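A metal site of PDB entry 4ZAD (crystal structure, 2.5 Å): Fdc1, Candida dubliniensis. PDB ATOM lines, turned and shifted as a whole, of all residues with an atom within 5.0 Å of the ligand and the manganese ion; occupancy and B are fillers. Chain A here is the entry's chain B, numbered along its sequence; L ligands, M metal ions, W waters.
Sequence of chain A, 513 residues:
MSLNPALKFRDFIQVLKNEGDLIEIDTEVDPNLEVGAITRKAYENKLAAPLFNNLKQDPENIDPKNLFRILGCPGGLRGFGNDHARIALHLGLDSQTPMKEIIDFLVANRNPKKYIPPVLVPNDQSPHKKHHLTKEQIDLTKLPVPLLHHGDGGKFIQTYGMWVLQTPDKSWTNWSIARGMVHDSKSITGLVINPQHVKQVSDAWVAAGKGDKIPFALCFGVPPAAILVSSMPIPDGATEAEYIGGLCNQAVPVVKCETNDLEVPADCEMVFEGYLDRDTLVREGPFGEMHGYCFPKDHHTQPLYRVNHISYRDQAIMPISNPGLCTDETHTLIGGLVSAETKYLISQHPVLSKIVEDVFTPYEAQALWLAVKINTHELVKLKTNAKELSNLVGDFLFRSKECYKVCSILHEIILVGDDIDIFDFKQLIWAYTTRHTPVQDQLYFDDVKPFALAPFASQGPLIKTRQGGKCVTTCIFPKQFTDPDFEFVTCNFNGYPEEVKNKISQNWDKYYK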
ATOM      1  N   GLN A 158     -16.553  19.779  -8.585  1.00  0.00           N
ATOM      2  CA  GLN A 158     -16.103  19.642  -9.967  1.00  0.00           C
ATOM      3  C   GLN A 158     -15.915  18.171 -10.364  1.00  0.00           C
ATOM      4  O   GLN A 158     -14.842  17.572 -10.117  1.00  0.00           O
ATOM      5  CB  GLN A 158     -14.832  20.489 -10.185  1.00  0.00           C
ATOM      6  CG  GLN A 158     -13.896  20.057 -11.312  1.00  0.00           C
ATOM      7  CD  GLN A 158     -14.579  19.922 -12.660  1.00  0.00           C
ATOM      8  OE1 GLN A 158     -15.806  19.850 -12.797  1.00  0.00           O
ATOM      9  NE2 GLN A 158     -13.770  19.888 -13.671  1.00  0.00           N
ATOM     10  N   THR A 159     -16.962  17.588 -10.943  1.00  0.00           N
ATOM     11  CA  THR A 159     -16.874  16.249 -11.541  1.00  0.00           C
ATOM     12  C   THR A 159     -17.337  16.176 -13.038  1.00  0.00           C
ATOM     13  O   THR A 159     -17.104  15.157 -13.705  1.00  0.00           O
ATOM     14  CB  THR A 159     -17.677  15.214 -10.770  1.00  0.00           C
ATOM     15  OG1 THR A 159     -19.077  15.547 -10.849  1.00  0.00           O
ATOM     16  CG2 THR A 159     -17.229  15.108  -9.291  1.00  0.00           C
ATOM     17  N   TYR A 160     -17.965  17.234 -13.556  1.00  0.00           N
ATOM     18  CA  TYR A 160     -18.236  17.329 -14.997  1.00  0.00           C
ATOM     19  C   TYR A 160     -18.169  18.762 -15.519  1.00  0.00           C
ATOM     20  O   TYR A 160     -18.889  19.133 -16.418  1.00  0.00           O
ATOM     21  CB  TYR A 160     -19.597  16.731 -15.340  1.00  0.00           C
ATOM     22  CG  TYR A 160     -19.741  16.112 -16.730  1.00  0.00           C
ATOM     23  CD1 TYR A 160     -19.058  14.935 -17.054  1.00  0.00           C
ATOM     24  CD2 TYR A 160     -20.632  16.626 -17.659  1.00  0.00           C
ATOM     25  CE1 TYR A 160     -19.212  14.321 -18.271  1.00  0.00           C
ATOM     26  CE2 TYR A 160     -20.788  16.014 -18.899  1.00  0.00           C
ATOM     27  CZ  TYR A 160     -20.069  14.850 -19.202  1.00  0.00           C
ATOM     28  OH  TYR A 160     -20.232  14.198 -20.436  1.00  0.00           O
ATOM     29  N   TRP A 172      -0.768  28.107 -26.019  1.00  0.00           N
ATOM     30  CA  TRP A 172      -1.564  26.904 -25.706  1.00  0.00           C
ATOM     31  C   TRP A 172      -2.611  27.185 -24.676  1.00  0.00           C
ATOM     32  O   TRP A 172      -2.272  27.665 -23.596  1.00  0.00           O
ATOM     33  CB  TRP A 172      -0.653  25.833 -25.117  1.00  0.00           C
ATOM     34  CG  TRP A 172      -1.314  24.547 -24.659  1.00  0.00           C
ATOM     35  CD1 TRP A 172      -2.592  24.122 -24.917  1.00  0.00           C
ATOM     36  CD2 TRP A 172      -0.680  23.504 -23.932  1.00  0.00           C
ATOM     37  NE1 TRP A 172      -2.792  22.891 -24.369  1.00  0.00           N
ATOM     38  CE2 TRP A 172      -1.641  22.479 -23.751  1.00  0.00           C
ATOM     39  CE3 TRP A 172       0.606  23.327 -23.413  1.00  0.00           C
ATOM     40  CZ2 TRP A 172      -1.364  21.306 -23.073  1.00  0.00           C
ATOM     41  CZ3 TRP A 172       0.886  22.167 -22.730  1.00  0.00           C
ATOM     42  CH2 TRP A 172      -0.103  21.162 -22.562  1.00  0.00           C
ATOM     43  N   ASN A 174      -5.676  25.085 -22.692  1.00  0.00           N
ATOM     44  CA  ASN A 174      -6.164  23.712 -22.449  1.00  0.00           C
ATOM     45  C   ASN A 174      -7.502  23.740 -21.760  1.00  0.00           C
ATOM     46  O   ASN A 174      -7.691  24.488 -20.798  1.00  0.00           O
ATOM     47  CB  ASN A 174      -5.166  22.932 -21.583  1.00  0.00           C
ATOM     48  CG  ASN A 174      -5.350  21.437 -21.708  1.00  0.00           C
ATOM     49  OD1 ASN A 174      -5.644  20.747 -20.723  1.00  0.00           O
ATOM     50  ND2 ASN A 174      -5.169  20.916 -22.923  1.00  0.00           N
ATOM     51  N   TRP A 175      -8.449  22.969 -22.310  1.00  0.00           N
ATOM     52  CA  TRP A 175      -9.708  22.639 -21.678  1.00  0.00           C
ATOM     53  C   TRP A 175      -9.698  21.175 -21.235  1.00  0.00           C
ATOM     54  O   TRP A 175      -9.500  20.284 -22.059  1.00  0.00           O
ATOM     55  CB  TRP A 175     -10.865  22.851 -22.644  1.00  0.00           C
ATOM     56  CG  TRP A 175     -11.111  24.263 -23.003  1.00  0.00           C
ATOM     57  CD1 TRP A 175     -10.415  25.357 -22.578  1.00  0.00           C
ATOM     58  CD2 TRP A 175     -12.110  24.741 -23.921  1.00  0.00           C
ATOM     59  NE1 TRP A 175     -10.954  26.489 -23.149  1.00  0.00           N
ATOM     60  CE2 TRP A 175     -11.987  26.138 -23.987  1.00  0.00           C
ATOM     61  CE3 TRP A 175     -13.114  24.122 -24.689  1.00  0.00           C
ATOM     62  CZ2 TRP A 175     -12.821  26.925 -24.778  1.00  0.00           C
ATOM     63  CZ3 TRP A 175     -13.940  24.903 -25.490  1.00  0.00           C
ATOM     64  CH2 TRP A 175     -13.784  26.295 -25.527  1.00  0.00           C
ATOM     65  N   SER A 176      -9.912  20.930 -19.940  1.00  0.00           N
ATOM     66  CA  SER A 176      -9.905  19.576 -19.439  1.00  0.00           C
ATOM     67  C   SER A 176     -10.772  19.335 -18.210  1.00  0.00           C
ATOM     68  O   SER A 176     -11.151  20.254 -17.492  1.00  0.00           O
ATOM     69  CB  SER A 176      -8.464  19.126 -19.174  1.00  0.00           C
ATOM     70  OG  SER A 176      -7.933  19.777 -18.029  1.00  0.00           O
ATOM     71  N   ILE A 177     -11.086  18.059 -17.959  1.00  0.00           N
ATOM     72  CA  ILE A 177     -11.713  17.669 -16.719  1.00  0.00           C
ATOM     73  C   ILE A 177     -10.632  17.170 -15.765  1.00  0.00           C
ATOM     74  O   ILE A 177      -9.815  16.295 -16.127  1.00  0.00           O
ATOM     75  CB  ILE A 177     -12.762  16.541 -16.862  1.00  0.00           C
ATOM     76  CG1 ILE A 177     -13.771  16.855 -17.957  1.00  0.00           C
ATOM     77  CG2 ILE A 177     -13.470  16.296 -15.499  1.00  0.00           C
ATOM     78  CD1 ILE A 177     -14.785  15.779 -18.146  1.00  0.00           C
ATOM     79  N   ALA A 178     -10.629  17.763 -14.577  1.00  0.00           N
ATOM     80  CA  ALA A 178      -9.988  17.145 -13.424  1.00  0.00           C
ATOM     81  C   ALA A 178     -10.935  17.368 -12.229  1.00  0.00           C
ATOM     82  O   ALA A 178     -11.640  18.384 -12.188  1.00  0.00           O
ATOM     83  CB  ALA A 178      -8.607  17.754 -13.186  1.00  0.00           C
ATOM     84  N   ARG A 179     -10.970  16.408 -11.313  1.00  0.00           N
ATOM     85  CA  ARG A 179     -11.864  16.445 -10.158  1.00  0.00           C
ATOM     86  C   ARG A 179     -11.430  17.531  -9.240  1.00  0.00           C
ATOM     87  O   ARG A 179     -10.229  17.809  -9.140  1.00  0.00           O
ATOM     88  CB  ARG A 179     -11.832  15.144  -9.346  1.00  0.00           C
ATOM     89  CG  ARG A 179     -10.614  14.978  -8.376  1.00  0.00           C
ATOM     90  CD  ARG A 179     -10.655  13.611  -7.732  1.00  0.00           C
ATOM     91  NE  ARG A 179      -9.639  13.370  -6.698  1.00  0.00           N
ATOM     92  CZ  ARG A 179      -9.075  12.179  -6.434  1.00  0.00           C
ATOM     93  NH1 ARG A 179      -9.364  11.065  -7.121  1.00  0.00           N
ATOM     94  NH2 ARG A 179      -8.173  12.086  -5.476  1.00  0.00           N
ATOM     95  N   LEU A 191      -7.105  17.420  -8.234  1.00  0.00           N
ATOM     96  CA  LEU A 191      -5.948  16.684  -8.806  1.00  0.00           C
ATOM     97  C   LEU A 191      -5.206  17.449  -9.933  1.00  0.00           C
ATOM     98  O   LEU A 191      -5.803  17.877 -10.918  1.00  0.00           O
ATOM     99  CB  LEU A 191      -6.353  15.300  -9.341  1.00  0.00           C
ATOM    100  CG  LEU A 191      -6.337  14.042  -8.477  1.00  0.00           C
ATOM    101  CD1 LEU A 191      -6.858  12.895  -9.336  1.00  0.00           C
ATOM    102  CD2 LEU A 191      -4.975  13.698  -7.912  1.00  0.00           C
ATOM    103  N   GLN A 196      -0.661  15.067 -16.705  1.00  0.00           N
ATOM    104  CA  GLN A 196      -1.885  15.726 -17.216  1.00  0.00           C
ATOM    105  C   GLN A 196      -1.657  17.196 -17.554  1.00  0.00           C
ATOM    106  O   GLN A 196      -0.785  17.834 -16.985  1.00  0.00           O
ATOM    107  CB  GLN A 196      -3.081  15.590 -16.256  1.00  0.00           C
ATOM    108  CG  GLN A 196      -3.533  14.127 -16.009  1.00  0.00           C
ATOM    109  CD  GLN A 196      -4.138  13.457 -17.230  1.00  0.00           C
ATOM    110  OE1 GLN A 196      -3.427  12.909 -18.069  1.00  0.00           O
ATOM    111  NE2 GLN A 196      -5.470  13.467 -17.335  1.00  0.00           N
ATOM    112  N   HIS A 197      -2.444  17.711 -18.471  1.00  0.00           N
ATOM    113  CA  HIS A 197      -2.180  19.044 -18.982  1.00  0.00           C
ATOM    114  C   HIS A 197      -2.443  20.106 -17.937  1.00  0.00           C
ATOM    115  O   HIS A 197      -1.770  21.116 -17.931  1.00  0.00           O
ATOM    116  CB  HIS A 197      -2.962  19.311 -20.252  1.00  0.00           C
ATOM    117  CG  HIS A 197      -2.440  18.568 -21.439  1.00  0.00           C
ATOM    118  ND1 HIS A 197      -3.211  18.310 -22.553  1.00  0.00           N
ATOM    119  CD2 HIS A 197      -1.219  18.011 -21.666  1.00  0.00           C
ATOM    120  CE1 HIS A 197      -2.486  17.639 -23.425  1.00  0.00           C
ATOM    121  NE2 HIS A 197      -1.277  17.436 -22.915  1.00  0.00           N
ATOM    122  N   VAL A 198      -3.387  19.875 -17.043  1.00  0.00           N
ATOM    123  CA  VAL A 198      -3.529  20.768 -15.916  1.00  0.00           C
ATOM    124  C   VAL A 198      -2.137  20.981 -15.299  1.00  0.00           C
ATOM    125  O   VAL A 198      -1.803  22.087 -14.920  1.00  0.00           O
ATOM    126  CB  VAL A 198      -4.570  20.248 -14.855  1.00  0.00           C
ATOM    127  CG1 VAL A 198      -4.209  18.852 -14.329  1.00  0.00           C
ATOM    128  CG2 VAL A 198      -4.658  21.202 -13.717  1.00  0.00           C
ATOM    129  N   SER A 230     -12.909  17.944 -23.628  1.00  0.00           N
ATOM    130  CA  SER A 230     -12.259  18.225 -22.360  1.00  0.00           C
ATOM    131  C   SER A 230     -11.723  16.892 -21.747  1.00  0.00           C
ATOM    132  O   SER A 230     -10.736  16.929 -20.981  1.00  0.00           O
ATOM    133  CB  SER A 230     -13.182  18.976 -21.383  1.00  0.00           C
ATOM    134  OG  SER A 230     -13.416  20.344 -21.739  1.00  0.00           O
ATOM    135  N   SER A 231     -12.333  15.724 -22.107  1.00  0.00           N
ATOM    136  CA  SER A 231     -11.912  14.410 -21.546  1.00  0.00           C
ATOM    137  C   SER A 231     -11.007  13.530 -22.386  1.00  0.00           C
ATOM    138  O   SER A 231     -10.737  12.396 -22.002  1.00  0.00           O
ATOM    139  CB  SER A 231     -13.123  13.544 -21.214  1.00  0.00           C
ATOM    140  OG  SER A 231     -14.198  14.345 -20.832  1.00  0.00           O
ATOM    141  N   MET A 232     -10.605  14.031 -23.538  1.00  0.00           N
ATOM    142  CA  MET A 232      -9.857  13.300 -24.554  1.00  0.00           C
ATOM    143  C   MET A 232      -8.438  13.780 -24.493  1.00  0.00           C
ATOM    144  O   MET A 232      -8.196  14.976 -24.529  1.00  0.00           O
ATOM    145  CB  MET A 232     -10.439  13.661 -25.928  1.00  0.00           C
ATOM    146  CG  MET A 232      -9.766  13.027 -27.139  1.00  0.00           C
ATOM    147  SD  MET A 232     -10.905  13.069 -28.564  1.00  0.00           S
ATOM    148  CE  MET A 232      -9.878  12.267 -29.800  1.00  0.00           C
ATOM    149  N   PRO A 233      -7.468  12.862 -24.435  1.00  0.00           N
ATOM    150  CA  PRO A 233      -6.079  13.298 -24.471  1.00  0.00           C
ATOM    151  C   PRO A 233      -5.582  13.683 -25.857  1.00  0.00           C
ATOM    152  O   PRO A 233      -4.834  12.923 -26.474  1.00  0.00           O
ATOM    153  CB  PRO A 233      -5.331  12.060 -23.953  1.00  0.00           C
ATOM    154  CG  PRO A 233      -6.112  10.939 -24.450  1.00  0.00           C
ATOM    155  CD  PRO A 233      -7.559  11.395 -24.425  1.00  0.00           C
ATOM    156  N   ILE A 234      -5.997  14.840 -26.374  1.00  0.00           N
ATOM    157  CA  ILE A 234      -5.408  15.348 -27.605  1.00  0.00           C
ATOM    158  C   ILE A 234      -3.987  15.850 -27.293  1.00  0.00           C
ATOM    159  O   ILE A 234      -3.599  15.991 -26.120  1.00  0.00           O
ATOM    160  CB  ILE A 234      -6.312  16.415 -28.313  1.00  0.00           C
ATOM    161  CG1 ILE A 234      -6.383  17.734 -27.537  1.00  0.00           C
ATOM    162  CG2 ILE A 234      -7.723  15.839 -28.589  1.00  0.00           C
ATOM    163  CD1 ILE A 234      -7.045  18.846 -28.348  1.00  0.00           C
ATOM    164  N   PRO A 235      -3.182  16.125 -28.318  1.00  0.00           N
ATOM    165  CA  PRO A 235      -1.758  16.220 -28.021  1.00  0.00           C
ATOM    166  C   PRO A 235      -1.313  17.320 -27.034  1.00  0.00           C
ATOM    167  O   PRO A 235      -2.056  18.300 -26.821  1.00  0.00           O
ATOM    168  CB  PRO A 235      -1.129  16.442 -29.415  1.00  0.00           C
ATOM    169  CG  PRO A 235      -2.118  15.849 -30.357  1.00  0.00           C
ATOM    170  CD  PRO A 235      -3.437  16.203 -29.768  1.00  0.00           C
ATOM    171  N   ALA A 238      -1.785  21.244 -27.864  1.00  0.00           N
ATOM    172  CA  ALA A 238      -2.907  21.395 -28.781  1.00  0.00           C
ATOM    173  C   ALA A 238      -4.079  22.064 -28.053  1.00  0.00           C
ATOM    174  O   ALA A 238      -4.399  21.686 -26.918  1.00  0.00           O
ATOM    175  CB  ALA A 238      -3.333  20.016 -29.336  1.00  0.00           C
ATOM    176  N   GLU A 240      -7.835  22.727 -27.431  1.00  0.00           N
ATOM    177  CA  GLU A 240      -9.016  21.898 -27.604  1.00  0.00           C
ATOM    178  C   GLU A 240     -10.112  22.628 -28.358  1.00  0.00           C
ATOM    179  O   GLU A 240     -10.810  22.013 -29.140  1.00  0.00           O
ATOM    180  CB  GLU A 240      -9.558  21.447 -26.239  1.00  0.00           C
ATOM    181  CG  GLU A 240      -8.877  20.226 -25.619  1.00  0.00           C
ATOM    182  CD  GLU A 240      -7.591  20.526 -24.819  1.00  0.00           C
ATOM    183  OE1 GLU A 240      -7.144  21.707 -24.737  1.00  0.00           O
ATOM    184  OE2 GLU A 240      -7.036  19.541 -24.251  1.00  0.00           O
ATOM    185  N   PHE A 287     -11.566   9.997  -3.057  1.00  0.00           N
ATOM    186  CA  PHE A 287     -12.766  10.082  -3.839  1.00  0.00           C
ATOM    187  C   PHE A 287     -13.064   8.744  -4.410  1.00  0.00           C
ATOM    188  O   PHE A 287     -12.180   8.076  -4.881  1.00  0.00           O
ATOM    189  CB  PHE A 287     -12.526  11.055  -4.949  1.00  0.00           C
ATOM    190  CG  PHE A 287     -13.731  11.404  -5.750  1.00  0.00           C
ATOM    191  CD1 PHE A 287     -14.922  11.771  -5.135  1.00  0.00           C
ATOM    192  CD2 PHE A 287     -13.653  11.436  -7.169  1.00  0.00           C
ATOM    193  CE1 PHE A 287     -16.035  12.144  -5.897  1.00  0.00           C
ATOM    194  CE2 PHE A 287     -14.747  11.804  -7.933  1.00  0.00           C
ATOM    195  CZ  PHE A 287     -15.937  12.160  -7.292  1.00  0.00           C
ATOM    196  N   GLU A 289     -13.572   6.509  -7.111  1.00  0.00           N
ATOM    197  CA  GLU A 289     -12.976   6.731  -8.435  1.00  0.00           C
ATOM    198  C   GLU A 289     -13.284   5.658  -9.522  1.00  0.00           C
ATOM    199  O   GLU A 289     -13.994   4.689  -9.299  1.00  0.00           O
ATOM    200  CB  GLU A 289     -11.482   7.052  -8.254  1.00  0.00           C
ATOM    201  CG  GLU A 289     -10.668   7.687  -9.520  1.00  0.00           C
ATOM    202  CD  GLU A 289     -11.212   9.001 -10.350  1.00  0.00           C
ATOM    203  OE1 GLU A 289     -11.176  10.160  -9.806  1.00  0.00           O
ATOM    204  OE2 GLU A 289     -11.467   8.845 -11.596  1.00  0.00           O
ATOM    205  N   SER A 321     -20.712  13.719 -12.530  1.00  0.00           N
ATOM    206  CA  SER A 321     -20.310  12.350 -12.755  1.00  0.00           C
ATOM    207  C   SER A 321     -19.916  11.729 -11.425  1.00  0.00           C
ATOM    208  O   SER A 321     -19.092  12.283 -10.698  1.00  0.00           O
ATOM    209  CB  SER A 321     -19.159  12.214 -13.737  1.00  0.00           C
ATOM    210  OG  SER A 321     -18.639  10.875 -13.703  1.00  0.00           O
ATOM    211  N   PRO A 323     -18.380   8.523 -10.360  1.00  0.00           N
ATOM    212  CA  PRO A 323     -17.653   7.335 -10.807  1.00  0.00           C
ATOM    213  C   PRO A 323     -17.733   6.099  -9.923  1.00  0.00           C
ATOM    214  O   PRO A 323     -17.931   6.202  -8.703  1.00  0.00           O
ATOM    215  CB  PRO A 323     -16.195   7.791 -10.820  1.00  0.00           C
ATOM    216  CG  PRO A 323     -16.239   9.232 -10.806  1.00  0.00           C
ATOM    217  CD  PRO A 323     -17.505   9.682 -10.175  1.00  0.00           C
ATOM    218  N   GLU A 329     -19.239   7.803 -16.807  1.00  0.00           N
ATOM    219  CA  GLU A 329     -18.459   8.713 -17.658  1.00  0.00           C
ATOM    220  C   GLU A 329     -16.969   8.399 -17.635  1.00  0.00           C
ATOM    221  O   GLU A 329     -16.264   8.663 -18.616  1.00  0.00           O
ATOM    222  CB  GLU A 329     -18.676  10.177 -17.232  1.00  0.00           C
ATOM    223  CG  GLU A 329     -20.086  10.685 -17.503  1.00  0.00           C
ATOM    224  CD  GLU A 329     -21.105  10.301 -16.475  1.00  0.00           C
ATOM    225  OE1 GLU A 329     -20.716   9.767 -15.424  1.00  0.00           O
ATOM    226  OE2 GLU A 329     -22.306  10.536 -16.706  1.00  0.00           O
ATOM    227  N   THR A 330     -16.479   7.826 -16.534  1.00  0.00           N
ATOM    228  CA  THR A 330     -15.090   7.437 -16.465  1.00  0.00           C
ATOM    229  C   THR A 330     -14.849   6.169 -17.269  1.00  0.00           C
ATOM    230  O   THR A 330     -13.738   5.677 -17.316  1.00  0.00           O
ATOM    231  CB  THR A 330     -14.573   7.300 -15.042  1.00  0.00           C
ATOM    232  OG1 THR A 330     -15.202   6.178 -14.400  1.00  0.00           O
ATOM    233  CG2 THR A 330     -14.833   8.592 -14.265  1.00  0.00           C
ATOM    234  N   LEU A 333     -16.339   8.071 -21.497  1.00  0.00           N
ATOM    235  CA  LEU A 333     -15.509   9.184 -21.891  1.00  0.00           C
ATOM    236  C   LEU A 333     -14.015   8.922 -21.650  1.00  0.00           C
ATOM    237  O   LEU A 333     -13.233   8.959 -22.573  1.00  0.00           O
ATOM    238  CB  LEU A 333     -15.976  10.483 -21.230  1.00  0.00           C
ATOM    239  CG  LEU A 333     -17.382  11.019 -21.598  1.00  0.00           C
ATOM    240  CD1 LEU A 333     -17.628  12.390 -21.003  1.00  0.00           C
ATOM    241  CD2 LEU A 333     -17.531  11.066 -23.142  1.00  0.00           C
ATOM    242  N   ILE A 334     -13.594   8.667 -20.426  1.00  0.00           N
ATOM    243  CA  ILE A 334     -12.182   8.431 -20.232  1.00  0.00           C
ATOM    244  C   ILE A 334     -11.685   7.327 -21.132  1.00  0.00           C
ATOM    245  O   ILE A 334     -10.681   7.492 -21.840  1.00  0.00           O
ATOM    246  CB  ILE A 334     -11.826   8.031 -18.792  1.00  0.00           C
ATOM    247  CG1 ILE A 334     -12.047   9.198 -17.826  1.00  0.00           C
ATOM    248  CG2 ILE A 334     -10.355   7.655 -18.743  1.00  0.00           C
ATOM    249  CD1 ILE A 334     -11.576   8.973 -16.394  1.00  0.00           C
ATOM    250  N   LYS A 405       1.297   9.658 -22.669  1.00  0.00           N
ATOM    251  CA  LYS A 405       0.204  10.207 -21.858  1.00  0.00           C
ATOM    252  C   LYS A 405      -1.181   9.596 -22.213  1.00  0.00           C
ATOM    253  O   LYS A 405      -1.894   9.039 -21.351  1.00  0.00           O
ATOM    254  CB  LYS A 405       0.143  11.713 -22.016  1.00  0.00           C
ATOM    255  CG  LYS A 405      -1.181  12.343 -21.472  1.00  0.00           C
ATOM    256  CD  LYS A 405      -1.079  13.848 -21.184  1.00  0.00           C
ATOM    257  CE  LYS A 405      -2.439  14.492 -21.061  1.00  0.00           C
ATOM    258  NZ  LYS A 405      -3.373  14.190 -22.182  1.00  0.00           N
HETATM  259  C1  LIG L   1     -12.510  12.499 -16.942  1.00  0.00           C
HETATM  260  C2  LIG L   1     -13.906  12.553 -16.791  1.00  0.00           C
HETATM  261  C3  LIG L   1     -14.497  12.617 -15.540  1.00  0.00           C
HETATM  262  C4  LIG L   1      -9.384  13.159 -15.068  1.00  0.00           C
HETATM  263  C5  LIG L   1     -13.581  12.624 -14.350  1.00  0.00           C
HETATM  264  N1  LIG L   1      -7.753  13.981 -13.021  1.00  0.00           N
HETATM  265  C6  LIG L   1      -7.287  13.856 -14.281  1.00  0.00           C
HETATM  266  C7  LIG L   1     -14.463  14.154 -12.692  1.00  0.00           C
HETATM  267  C8  LIG L   1     -14.062  12.720 -13.001  1.00  0.00           C
HETATM  268  C9  LIG L   1     -11.691  12.548 -12.317  1.00  0.00           C
HETATM  269  O1  LIG L   1      -6.098  14.135 -14.461  1.00  0.00           O
HETATM  270  N2  LIG L   1      -8.095  13.455 -15.304  1.00  0.00           N
HETATM  271  C10 LIG L   1      -9.054  13.668 -12.776  1.00  0.00           C
HETATM  272  O2  LIG L   1      -9.438  13.784 -11.592  1.00  0.00           O
HETATM  273  C11 LIG L   1      -9.871  13.257 -13.772  1.00  0.00           C
HETATM  274  N3  LIG L   1     -11.240  12.532 -13.527  1.00  0.00           N
HETATM  275  C12 LIG L   1     -13.025  12.627 -12.024  1.00  0.00           C
HETATM  276  C13 LIG L   1     -15.152  11.683 -12.759  1.00  0.00           C
HETATM  277  C14 LIG L   1     -12.105  12.557 -14.587  1.00  0.00           C
HETATM  278  C15 LIG L   1     -15.999  12.693 -15.453  1.00  0.00           C
HETATM  279  C16 LIG L   1     -14.821  12.550 -17.971  1.00  0.00           C
HETATM  280  C17 LIG L   1     -11.603  12.473 -15.868  1.00  0.00           C
HETATM  281  N4  LIG L   1     -10.208  12.768 -16.070  1.00  0.00           N
HETATM  282  C18 LIG L   1      -9.492  12.298 -17.262  1.00  0.00           C
HETATM  283  C19 LIG L   1      -9.092  13.544 -18.057  1.00  0.00           C
HETATM  284  O3  LIG L   1     -10.166  14.516 -18.126  1.00  0.00           O
HETATM  285  C20 LIG L   1      -8.535  13.089 -19.409  1.00  0.00           C
HETATM  286  O4  LIG L   1      -7.333  12.341 -19.218  1.00  0.00           O
HETATM  287  C21 LIG L   1      -8.171  14.260 -20.300  1.00  0.00           C
HETATM  288  O5  LIG L   1      -7.424  13.728 -21.389  1.00  0.00           O
HETATM  289  C22 LIG L   1      -7.345  15.328 -19.588  1.00  0.00           C
HETATM  290  O6  LIG L   1      -7.258  16.495 -20.394  1.00  0.00           O
HETATM  291  P1  LIG L   1      -5.862  16.855 -21.041  1.00  0.00           P
HETATM  292  O7  LIG L   1      -6.084  18.199 -21.704  1.00  0.00           O
HETATM  293  O8  LIG L   1      -5.677  15.741 -22.052  1.00  0.00           O
HETATM  294  O9  LIG L   1      -4.875  16.824 -19.894  1.00  0.00           O
HETATM  295 MN    MN M   1      -5.134  18.969 -23.518  1.00  0.00          MN
HETATM  296  O   HOH W   1      -5.399  17.038 -24.431  1.00  0.00           O
HETATM  297  O   HOH W   2      -4.031  19.696 -25.356  1.00  0.00           O
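An oxygen (O4) of the ligand sits at hydrogen-bond distance from the side-chain amide nitrogen (NE2) of Gln 196 (2.9 Å). O9 of the ligand sits at hydrogen-bond distance from N of His 197. O8 of the ligand is in salt-bridge range of NZ of Lys 405, 2.8 Å away. O of Ile 177 sits at hydrogen-bond distance from O3 of the ligand (2.7 Å). An oxygen (O2) of the ligand lies within hydrogen-bond range of the backbone NH (N) of Arg 179. The backbone carbonyl oxygen (O) of Met 232 sits close to an oxygen (O5) of the ligand (3.5 Å).
The backbone carbonyl oxygen of Arg 179 sits at hydrogen-bond distance from the backbone NH of Leu 191 (3.3 Å). N of Ile 334 sits at hydrogen-bond distance from O of Glu 329, at 3.2 Å. The backbone carbonyl oxygen (O) of Ala 178 lies close to the side-chain amide nitrogen (NE2) of Gln 158, at 3.0 Å. The side-chain carboxylate (OE1) of Glu 289 is in salt-bridge range of the guanidinium group (NH1) of Arg 179, 3.4 Å away. The side-chain carboxylate (OE1) of Glu 240 is in hydrogen-bond range of the backbone NH (N) of Trp 175. The side-chain hydroxyl (OG1) of Thr 159 is in hydrogen-bond range of the backbone NH (N) of Ser 321 (3.0 Å). The side-chain hydroxyl of Ser 321 sits at hydrogen-bond distance from the side-chain carboxylate of Glu 329. N of Ile 177 sits at hydrogen-bond distance from O of Ser 230, at 3.2 Å.
The backbone nitrogen of Pro 233 sits close to an oxygen (O5) of the ligand (3.2 Å). Merely in contact with the ligand: Thr 159, Ser 176, Ala 178, Leu 191, Ser 230, Ser 231, Glu 289, Ser 321, Pro 323, Thr 330 and Ile 334. Hydrophobic or aromatic side chains that line the ligand: Ile 177, Ala 178, Leu 191, His 197, Pro 233, Pro 323 and Ile 334. 20 residues have an atom within 4 Å of the ligand: Thr 159, Asn 174, Ser 176, Ile 177, Ala 178, Arg 179, Leu 191, Gln 196, His 197, Ser 230, Ser 231, Met 232, Pro 233, Glu 240, Glu 289, Ser 321, Pro 323, Thr 330, Ile 334 and Lys 405. The nearest printed residue that does not touch the ligand is Trp 175 (4.02 Å).
Of the 31 residues printed, 3 come within 4 Å of the manganese ion. Along chain A the residues within 4 Å of the manganese ion span positions 174 to 240. The nearest printed residue that does not touch the manganese ion is Ile 234 (4.2 Å).
The manganese ion is bound by the side-chain amide nitrogen (ND2) of Asn 174 (2.0 Å), the side-chain carboxylate (OE2) of Glu 240 (2.1 Å), water W1 (2.2 Å), an oxygen (O7) of the ligand (2.2 Å), a ring nitrogen (ND1) of His 197 (2.3 Å) and water W2 (2.3 Å). The manganese ion has six donor atoms within binding distance.
Water W1 lies within hydrogen-bond range of the backbone carbonyl oxygen of Ile 234, an oxygen (O8) of the ligand and the backbone carbonyl oxygen of Met 232.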
